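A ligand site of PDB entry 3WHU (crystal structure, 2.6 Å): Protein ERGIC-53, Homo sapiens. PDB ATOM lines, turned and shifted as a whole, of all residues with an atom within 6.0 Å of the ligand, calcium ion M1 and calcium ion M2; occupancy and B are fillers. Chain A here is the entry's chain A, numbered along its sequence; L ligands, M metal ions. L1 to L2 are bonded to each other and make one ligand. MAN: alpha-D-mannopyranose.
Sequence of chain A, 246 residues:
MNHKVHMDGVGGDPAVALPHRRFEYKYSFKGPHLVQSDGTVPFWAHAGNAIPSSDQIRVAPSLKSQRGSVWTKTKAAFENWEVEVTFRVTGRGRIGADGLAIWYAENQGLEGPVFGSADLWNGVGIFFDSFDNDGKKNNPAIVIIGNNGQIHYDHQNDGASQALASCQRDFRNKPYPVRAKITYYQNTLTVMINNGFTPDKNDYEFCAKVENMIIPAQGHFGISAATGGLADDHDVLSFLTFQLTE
The side-chain amide nitrogen of Asn 133 sits at hydrogen-bond distance from an oxygen (O4) of MAN L1 (3.0 Å).
An oxygen (O6) of MAN L1 is in hydrogen-bond range of the backbone NH (N) of Gly 229, at 2.8 Å.
O4 of MAN L1 sits at hydrogen-bond distance from OD2 of Asp 98 (2.9 Å).
N of Leu 230 sits at hydrogen-bond distance from O6 of MAN L1, 3.2 Å away.
The backbone carbonyl oxygen (O) of Leu 230 lies within hydrogen-bond range of an oxygen (O6) of MAN L1 (3.4 Å).
O6 of MAN L1 sits at hydrogen-bond distance from N of Gly 228 (3.3 Å).
The side-chain hydroxyl of Ser 65 is in hydrogen-bond range of an oxygen (O4) of MAN L2, 3.4 Å away.
A ring nitrogen (NE2) of His 155 is in hydrogen-bond range of an oxygen (O3) of MAN L1 (3.5 Å).
ND2 of Asn 139 sits at hydrogen-bond distance from O of Asp 129 (3.2 Å).
The side-chain amide nitrogen of Asn 139 sits close to the backbone carbonyl oxygen of Phe 131, at 2.8 Å.
The side-chain amide oxygen (OD1) of Asn 139 lies close to the side-chain amide oxygen (OD1) of Asn 138 (3.3 Å).
A ring nitrogen (NE2) of His 155 is in hydrogen-bond range of the side-chain carboxylate (OD1) of Asp 98 (3.5 Å).
The backbone carbonyl oxygen (O) of Asp 98 lies within hydrogen-bond range of the backbone NH (N) of Ser 130.
The side-chain amide nitrogen (ND2) of Asn 139 sits close to the backbone NH (N) of Asp 132 (3.3 Å).
The backbone NH (N) of Ser 65 is in hydrogen-bond range of the backbone carbonyl oxygen (O) of Gly 228 (3.1 Å).
The backbone NH (N) of Ser 65 lies within hydrogen-bond range of the side-chain hydroxyl (OG1) of Thr 227 (3.1 Å).
Residues that only touch the ligand: Ala 97 (3.4 Å).
Hydrophobic or aromatic side chains that line the ligand: Ala 97, Phe 131 and His 155.
Within 4 Å of the ligand: Ser 65, Ala 97, Asp 98, Phe 131, Asn 133, His 155, Gly 228, Gly 229 and Leu 230.
Along chain A the residues within 4 Å of the ligand span positions 65 to 230.
Four residues have an atom within 4 Å of calcium ion M1: Asp 129, Phe 131, Asn 133 and Asp 158.
Asp 132 touches calcium ion M2 (OD1 to CA, 3.4 Å).
Of the 25 residues printed, 5 come within 4 Å of calcium ion M2.
The nearest printed residue that does not touch calcium ion M2 is Asn 133 (4.6 Å).
Calcium ion M1 is bound by the side-chain amide oxygen (OD1) of Asn 133, the side-chain carboxylate (OD1) of Asp 158, the side-chain carboxylate (OD1) of Asp 129, the side-chain carboxylate (OD2) of Asp 129 and the backbone carbonyl oxygen (O) of Phe 131.
Calcium ion M1 has five donor atoms within binding distance.
Calcium ion M2 is bound by the side-chain carboxylate of Asp 158 (2.2 Å), the side-chain carboxylate of Asp 134 (2.6 Å), the side-chain amide oxygen of Asn 138 (2.8 Å) and the side-chain amide nitrogen of Asn 138 (2.9 Å).
Slightly farther from calcium ion M2 lies the side-chain amide oxygen (OD1) of Asn 139 (3.1 Å).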
ATOM      1  N   SER A  65      19.877 -23.600 -20.099  1.00  0.00           N
ATOM      2  CA  SER A  65      19.304 -24.482 -19.099  1.00  0.00           C
ATOM      3  C   SER A  65      20.149 -25.756 -18.941  1.00  0.00           C
ATOM      4  O   SER A  65      19.669 -26.872 -19.120  1.00  0.00           O
ATOM      5  CB  SER A  65      17.834 -24.804 -19.467  1.00  0.00           C
ATOM      6  OG  SER A  65      17.152 -23.687 -20.061  1.00  0.00           O
ATOM      7  N   GLY A  96      26.490 -12.743 -17.793  1.00  0.00           N
ATOM      8  CA  GLY A  96      26.370 -14.166 -18.048  1.00  0.00           C
ATOM      9  C   GLY A  96      25.683 -14.898 -16.928  1.00  0.00           C
ATOM     10  O   GLY A  96      25.412 -14.353 -15.867  1.00  0.00           O
ATOM     11  N   ALA A  97      25.390 -16.168 -17.171  1.00  0.00           N
ATOM     12  CA  ALA A  97      24.775 -17.001 -16.162  1.00  0.00           C
ATOM     13  C   ALA A  97      25.256 -18.413 -16.362  1.00  0.00           C
ATOM     14  O   ALA A  97      25.885 -18.682 -17.387  1.00  0.00           O
ATOM     15  CB  ALA A  97      23.275 -16.958 -16.309  1.00  0.00           C
ATOM     16  N   ASP A  98      24.986 -19.296 -15.388  1.00  0.00           N
ATOM     17  CA  ASP A  98      24.430 -18.891 -14.078  1.00  0.00           C
ATOM     18  C   ASP A  98      25.506 -18.869 -12.977  1.00  0.00           C
ATOM     19  O   ASP A  98      25.418 -18.072 -12.012  1.00  0.00           O
ATOM     20  CB  ASP A  98      23.268 -19.804 -13.657  1.00  0.00           C
ATOM     21  CG  ASP A  98      21.999 -19.024 -13.336  1.00  0.00           C
ATOM     22  OD1 ASP A  98      20.918 -19.669 -13.329  1.00  0.00           O
ATOM     23  OD2 ASP A  98      22.055 -17.782 -13.095  1.00  0.00           O
ATOM     24  N   PHE A 115      23.008 -24.501  -8.444  1.00  0.00           N
ATOM     25  CA  PHE A 115      24.083 -24.451  -9.416  1.00  0.00           C
ATOM     26  C   PHE A 115      24.408 -25.855  -9.941  1.00  0.00           C
ATOM     27  O   PHE A 115      25.549 -26.347  -9.860  1.00  0.00           O
ATOM     28  CB  PHE A 115      25.289 -23.779  -8.786  1.00  0.00           C
ATOM     29  CG  PHE A 115      25.082 -22.309  -8.558  1.00  0.00           C
ATOM     30  CD1 PHE A 115      25.653 -21.374  -9.396  1.00  0.00           C
ATOM     31  CD2 PHE A 115      24.291 -21.865  -7.514  1.00  0.00           C
ATOM     32  CE1 PHE A 115      25.450 -20.030  -9.215  1.00  0.00           C
ATOM     33  CE2 PHE A 115      24.092 -20.505  -7.315  1.00  0.00           C
ATOM     34  CZ  PHE A 115      24.667 -19.587  -8.167  1.00  0.00           C
ATOM     35  N   ASP A 129      28.702 -16.606  -8.445  1.00  0.00           N
ATOM     36  CA  ASP A 129      27.381 -16.280  -8.972  1.00  0.00           C
ATOM     37  C   ASP A 129      27.465 -15.162 -10.000  1.00  0.00           C
ATOM     38  O   ASP A 129      27.660 -14.001  -9.678  1.00  0.00           O
ATOM     39  CB  ASP A 129      26.461 -15.905  -7.822  1.00  0.00           C
ATOM     40  CG  ASP A 129      25.010 -15.869  -8.214  1.00  0.00           C
ATOM     41  OD1 ASP A 129      24.701 -15.627  -9.410  1.00  0.00           O
ATOM     42  OD2 ASP A 129      24.149 -16.062  -7.313  1.00  0.00           O
ATOM     43  N   SER A 130      27.308 -15.545 -11.262  1.00  0.00           N
ATOM     44  CA  SER A 130      27.501 -14.639 -12.372  1.00  0.00           C
ATOM     45  C   SER A 130      26.299 -13.729 -12.502  1.00  0.00           C
ATOM     46  O   SER A 130      26.398 -12.624 -13.050  1.00  0.00           O
ATOM     47  CB  SER A 130      27.684 -15.432 -13.675  1.00  0.00           C
ATOM     48  OG  SER A 130      28.336 -16.680 -13.480  1.00  0.00           O
ATOM     49  N   PHE A 131      25.145 -14.228 -12.041  1.00  0.00           N
ATOM     50  CA  PHE A 131      23.862 -13.602 -12.347  1.00  0.00           C
ATOM     51  C   PHE A 131      23.158 -12.930 -11.159  1.00  0.00           C
ATOM     52  O   PHE A 131      22.766 -13.580 -10.187  1.00  0.00           O
ATOM     53  CB  PHE A 131      22.914 -14.582 -13.049  1.00  0.00           C
ATOM     54  CG  PHE A 131      21.780 -13.881 -13.760  1.00  0.00           C
ATOM     55  CD1 PHE A 131      22.042 -12.888 -14.705  1.00  0.00           C
ATOM     56  CD2 PHE A 131      20.460 -14.170 -13.449  1.00  0.00           C
ATOM     57  CE1 PHE A 131      21.009 -12.223 -15.335  1.00  0.00           C
ATOM     58  CE2 PHE A 131      19.414 -13.488 -14.069  1.00  0.00           C
ATOM     59  CZ  PHE A 131      19.695 -12.523 -15.016  1.00  0.00           C
ATOM     60  N   ASP A 132      22.988 -11.617 -11.313  1.00  0.00           N
ATOM     61  CA  ASP A 132      22.318 -10.769 -10.330  1.00  0.00           C
ATOM     62  C   ASP A 132      20.781 -11.035 -10.283  1.00  0.00           C
ATOM     63  O   ASP A 132      19.997 -10.257 -10.837  1.00  0.00           O
ATOM     64  CB  ASP A 132      22.626  -9.294 -10.687  1.00  0.00           C
ATOM     65  CG  ASP A 132      22.239  -8.312  -9.600  1.00  0.00           C
ATOM     66  OD1 ASP A 132      22.425  -8.625  -8.400  1.00  0.00           O
ATOM     67  OD2 ASP A 132      21.757  -7.213  -9.963  1.00  0.00           O
ATOM     68  N   ASN A 133      20.357 -12.119  -9.634  1.00  0.00           N
ATOM     69  CA  ASN A 133      18.940 -12.544  -9.630  1.00  0.00           C
ATOM     70  C   ASN A 133      17.976 -11.682  -8.774  1.00  0.00           C
ATOM     71  O   ASN A 133      16.779 -11.609  -9.054  1.00  0.00           O
ATOM     72  CB  ASN A 133      18.793 -13.997  -9.157  1.00  0.00           C
ATOM     73  CG  ASN A 133      19.566 -14.981 -10.025  1.00  0.00           C
ATOM     74  OD1 ASN A 133      20.759 -14.790 -10.286  1.00  0.00           O
ATOM     75  ND2 ASN A 133      18.901 -16.062 -10.437  1.00  0.00           N
ATOM     76  N   ASP A 134      18.500 -11.072  -7.719  1.00  0.00           N
ATOM     77  CA  ASP A 134      17.718 -10.177  -6.861  1.00  0.00           C
ATOM     78  C   ASP A 134      18.153  -8.730  -7.119  1.00  0.00           C
ATOM     79  O   ASP A 134      18.419  -7.970  -6.179  1.00  0.00           O
ATOM     80  CB  ASP A 134      17.856 -10.569  -5.376  1.00  0.00           C
ATOM     81  CG  ASP A 134      19.315 -10.657  -4.899  1.00  0.00           C
ATOM     82  OD1 ASP A 134      20.169  -9.896  -5.402  1.00  0.00           O
ATOM     83  OD2 ASP A 134      19.613 -11.480  -4.022  1.00  0.00           O
ATOM     84  N   GLY A 135      18.249  -8.364  -8.401  1.00  0.00           N
ATOM     85  CA  GLY A 135      18.371  -6.967  -8.836  1.00  0.00           C
ATOM     86  C   GLY A 135      19.181  -5.981  -8.007  1.00  0.00           C
ATOM     87  O   GLY A 135      18.969  -4.789  -8.135  1.00  0.00           O
ATOM     88  N   LYS A 136      20.117  -6.469  -7.191  1.00  0.00           N
ATOM     89  CA  LYS A 136      20.902  -5.612  -6.279  1.00  0.00           C
ATOM     90  C   LYS A 136      22.201  -5.051  -6.884  1.00  0.00           C
ATOM     91  O   LYS A 136      23.003  -4.496  -6.146  1.00  0.00           O
ATOM     92  CB  LYS A 136      21.254  -6.381  -4.982  1.00  0.00           C
ATOM     93  CG  LYS A 136      20.204  -6.364  -3.878  1.00  0.00           C
ATOM     94  CD  LYS A 136      20.190  -5.042  -3.117  1.00  0.00           C
ATOM     95  CE  LYS A 136      19.056  -4.991  -2.086  1.00  0.00           C
ATOM     96  NZ  LYS A 136      18.687  -3.610  -1.639  1.00  0.00           N
ATOM     97  N   ASN A 138      24.926  -6.364  -7.397  1.00  0.00           N
ATOM     98  CA  ASN A 138      25.944  -6.876  -6.479  1.00  0.00           C
ATOM     99  C   ASN A 138      26.683  -8.132  -7.005  1.00  0.00           C
ATOM    100  O   ASN A 138      27.269  -8.884  -6.217  1.00  0.00           O
ATOM    101  CB  ASN A 138      25.296  -7.212  -5.109  1.00  0.00           C
ATOM    102  CG  ASN A 138      24.113  -8.166  -5.241  1.00  0.00           C
ATOM    103  OD1 ASN A 138      23.471  -8.253  -6.310  1.00  0.00           O
ATOM    104  ND2 ASN A 138      23.810  -8.877  -4.170  1.00  0.00           N
ATOM    105  N   ASN A 139      26.630  -8.340  -8.339  1.00  0.00           N
ATOM    106  CA  ASN A 139      27.178  -9.546  -8.990  1.00  0.00           C
ATOM    107  C   ASN A 139      28.127  -9.187 -10.140  1.00  0.00           C
ATOM    108  O   ASN A 139      28.016  -8.098 -10.697  1.00  0.00           O
ATOM    109  CB  ASN A 139      26.038 -10.434  -9.519  1.00  0.00           C
ATOM    110  CG  ASN A 139      25.383 -11.274  -8.430  1.00  0.00           C
ATOM    111  OD1 ASN A 139      25.234 -10.836  -7.283  1.00  0.00           O
ATOM    112  ND2 ASN A 139      24.974 -12.479  -8.785  1.00  0.00           N
ATOM    113  N   TYR A 153      18.138 -23.356  -0.945  1.00  0.00           N
ATOM    114  CA  TYR A 153      18.941 -22.255  -1.492  1.00  0.00           C
ATOM    115  C   TYR A 153      18.057 -21.221  -2.226  1.00  0.00           C
ATOM    116  O   TYR A 153      17.268 -21.578  -3.117  1.00  0.00           O
ATOM    117  CB  TYR A 153      20.104 -22.754  -2.393  1.00  0.00           C
ATOM    118  CG  TYR A 153      20.636 -21.654  -3.263  1.00  0.00           C
ATOM    119  CD1 TYR A 153      21.286 -20.563  -2.699  1.00  0.00           C
ATOM    120  CD2 TYR A 153      20.428 -21.662  -4.633  1.00  0.00           C
ATOM    121  CE1 TYR A 153      21.750 -19.516  -3.491  1.00  0.00           C
ATOM    122  CE2 TYR A 153      20.884 -20.627  -5.434  1.00  0.00           C
ATOM    123  CZ  TYR A 153      21.550 -19.548  -4.858  1.00  0.00           C
ATOM    124  OH  TYR A 153      21.997 -18.511  -5.665  1.00  0.00           O
ATOM    125  N   HIS A 155      17.601 -19.262  -4.672  1.00  0.00           N
ATOM    126  CA  HIS A 155      18.110 -18.982  -6.003  1.00  0.00           C
ATOM    127  C   HIS A 155      17.828 -17.561  -6.404  1.00  0.00           C
ATOM    128  O   HIS A 155      18.754 -16.809  -6.663  1.00  0.00           O
ATOM    129  CB  HIS A 155      17.562 -19.937  -7.067  1.00  0.00           C
ATOM    130  CG  HIS A 155      18.318 -19.892  -8.355  1.00  0.00           C
ATOM    131  ND1 HIS A 155      19.292 -20.817  -8.687  1.00  0.00           N
ATOM    132  CD2 HIS A 155      18.288 -18.999  -9.375  1.00  0.00           C
ATOM    133  CE1 HIS A 155      19.800 -20.510  -9.867  1.00  0.00           C
ATOM    134  NE2 HIS A 155      19.210 -19.414 -10.308  1.00  0.00           N
ATOM    135  N   ASN A 157      17.089 -15.047  -4.790  1.00  0.00           N
ATOM    136  CA  ASN A 157      17.781 -14.064  -3.949  1.00  0.00           C
ATOM    137  C   ASN A 157      19.278 -14.334  -3.726  1.00  0.00           C
ATOM    138  O   ASN A 157      19.843 -13.836  -2.744  1.00  0.00           O
ATOM    139  CB  ASN A 157      17.070 -13.895  -2.597  1.00  0.00           C
ATOM    140  CG  ASN A 157      15.813 -13.060  -2.705  1.00  0.00           C
ATOM    141  OD1 ASN A 157      15.878 -11.867  -3.013  1.00  0.00           O
ATOM    142  ND2 ASN A 157      14.666 -13.673  -2.459  1.00  0.00           N
ATOM    143  N   ASP A 158      19.914 -15.079  -4.629  1.00  0.00           N
ATOM    144  CA  ASP A 158      21.363 -15.259  -4.583  1.00  0.00           C
ATOM    145  C   ASP A 158      21.808 -15.564  -3.151  1.00  0.00           C
ATOM    146  O   ASP A 158      22.776 -14.986  -2.659  1.00  0.00           O
ATOM    147  CB  ASP A 158      22.066 -13.980  -5.076  1.00  0.00           C
ATOM    148  CG  ASP A 158      21.837 -13.718  -6.576  1.00  0.00           C
ATOM    149  OD1 ASP A 158      21.685 -14.704  -7.332  1.00  0.00           O
ATOM    150  OD2 ASP A 158      21.834 -12.532  -7.002  1.00  0.00           O
ATOM    151  N   ALA A 160      21.351 -14.379  -0.381  1.00  0.00           N
ATOM    152  CA  ALA A 160      21.929 -13.265   0.389  1.00  0.00           C
ATOM    153  C   ALA A 160      21.660 -13.397   1.894  1.00  0.00           C
ATOM    154  O   ALA A 160      22.528 -13.133   2.707  1.00  0.00           O
ATOM    155  CB  ALA A 160      21.471 -11.915  -0.158  1.00  0.00           C
ATOM    156  N   THR A 227      23.364 -23.105 -16.202  1.00  0.00           N
ATOM    157  CA  THR A 227      22.916 -21.971 -17.000  1.00  0.00           C
ATOM    158  C   THR A 227      21.391 -21.997 -17.044  1.00  0.00           C
ATOM    159  O   THR A 227      20.756 -22.928 -16.561  1.00  0.00           O
ATOM    160  CB  THR A 227      23.455 -22.122 -18.454  1.00  0.00           C
ATOM    161  OG1 THR A 227      22.812 -23.237 -19.087  1.00  0.00           O
ATOM    162  CG2 THR A 227      24.995 -22.327 -18.465  1.00  0.00           C
ATOM    163  N   GLY A 228      20.807 -20.974 -17.637  1.00  0.00           N
ATOM    164  CA  GLY A 228      19.379 -20.969 -17.900  1.00  0.00           C
ATOM    165  C   GLY A 228      19.055 -20.139 -19.119  1.00  0.00           C
ATOM    166  O   GLY A 228      19.305 -20.551 -20.260  1.00  0.00           O
ATOM    167  N   GLY A 229      18.485 -18.960 -18.875  1.00  0.00           N
ATOM    168  CA  GLY A 229      18.173 -18.057 -19.958  1.00  0.00           C
ATOM    169  C   GLY A 229      19.453 -17.621 -20.632  1.00  0.00           C
ATOM    170  O   GLY A 229      19.584 -17.699 -21.866  1.00  0.00           O
ATOM    171  N   LEU A 230      20.394 -17.160 -19.817  1.00  0.00           N
ATOM    172  CA  LEU A 230      21.752 -16.868 -20.254  1.00  0.00           C
ATOM    173  C   LEU A 230      22.672 -18.050 -19.943  1.00  0.00           C
ATOM    174  O   LEU A 230      22.326 -18.888 -19.102  1.00  0.00           O
ATOM    175  CB  LEU A 230      22.248 -15.609 -19.548  1.00  0.00           C
ATOM    176  CG  LEU A 230      21.313 -14.416 -19.706  1.00  0.00           C
ATOM    177  CD1 LEU A 230      21.677 -13.313 -18.727  1.00  0.00           C
ATOM    178  CD2 LEU A 230      21.354 -13.907 -21.135  1.00  0.00           C
ATOM    179  N   ALA A 231      23.809 -18.153 -20.623  1.00  0.00           N
ATOM    180  CA  ALA A 231      24.653 -19.334 -20.483  1.00  0.00           C
ATOM    181  C   ALA A 231      26.123 -19.077 -20.788  1.00  0.00           C
ATOM    182  O   ALA A 231      26.451 -18.559 -21.856  1.00  0.00           O
ATOM    183  CB  ALA A 231      24.130 -20.455 -21.392  1.00  0.00           C
HETATM  184  C1  MAN L   1      16.277 -17.027 -16.167  1.00  0.00           C
HETATM  185  C2  MAN L   1      16.095 -17.910 -14.911  1.00  0.00           C
HETATM  186  C3  MAN L   1      17.037 -17.634 -13.756  1.00  0.00           C
HETATM  187  C4  MAN L   1      18.458 -17.458 -14.290  1.00  0.00           C
HETATM  188  C5  MAN L   1      18.554 -16.520 -15.490  1.00  0.00           C
HETATM  189  C6  MAN L   1      19.926 -16.632 -16.150  1.00  0.00           C
HETATM  190  O1  MAN L   1      15.645 -15.775 -16.028  1.00  0.00           O
HETATM  191  O2  MAN L   1      16.306 -19.291 -15.166  1.00  0.00           O
HETATM  192  O3  MAN L   1      16.972 -18.767 -12.890  1.00  0.00           O
HETATM  193  O4  MAN L   1      19.275 -16.963 -13.250  1.00  0.00           O
HETATM  194  O5  MAN L   1      17.631 -16.781 -16.515  1.00  0.00           O
HETATM  195  O6  MAN L   1      20.062 -17.919 -16.759  1.00  0.00           O
HETATM  196  C1  MAN L   2      15.066 -19.967 -15.094  1.00  0.00           C
HETATM  197  C2  MAN L   2      15.179 -21.501 -15.239  1.00  0.00           C
HETATM  198  C3  MAN L   2      15.514 -21.910 -16.697  1.00  0.00           C
HETATM  199  C4  MAN L   2      14.456 -21.250 -17.604  1.00  0.00           C
HETATM  200  C5  MAN L   2      14.655 -19.721 -17.457  1.00  0.00           C
HETATM  201  C6  MAN L   2      13.879 -18.853 -18.469  1.00  0.00           C
HETATM  202  O2  MAN L   2      13.950 -22.094 -14.767  1.00  0.00           O
HETATM  203  O3  MAN L   2      15.574 -23.325 -16.929  1.00  0.00           O
HETATM  204  O4  MAN L   2      14.558 -21.753 -18.929  1.00  0.00           O
HETATM  205  O5  MAN L   2      14.305 -19.360 -16.124  1.00  0.00           O
HETATM  206  O6  MAN L   2      12.488 -19.024 -18.229  1.00  0.00           O
HETATM  207 CA    CA M   1      22.167 -15.944  -9.095  1.00  0.00          CA
HETATM  208 CA    CA M   2      22.527 -10.817  -5.821  1.00  0.00          CA
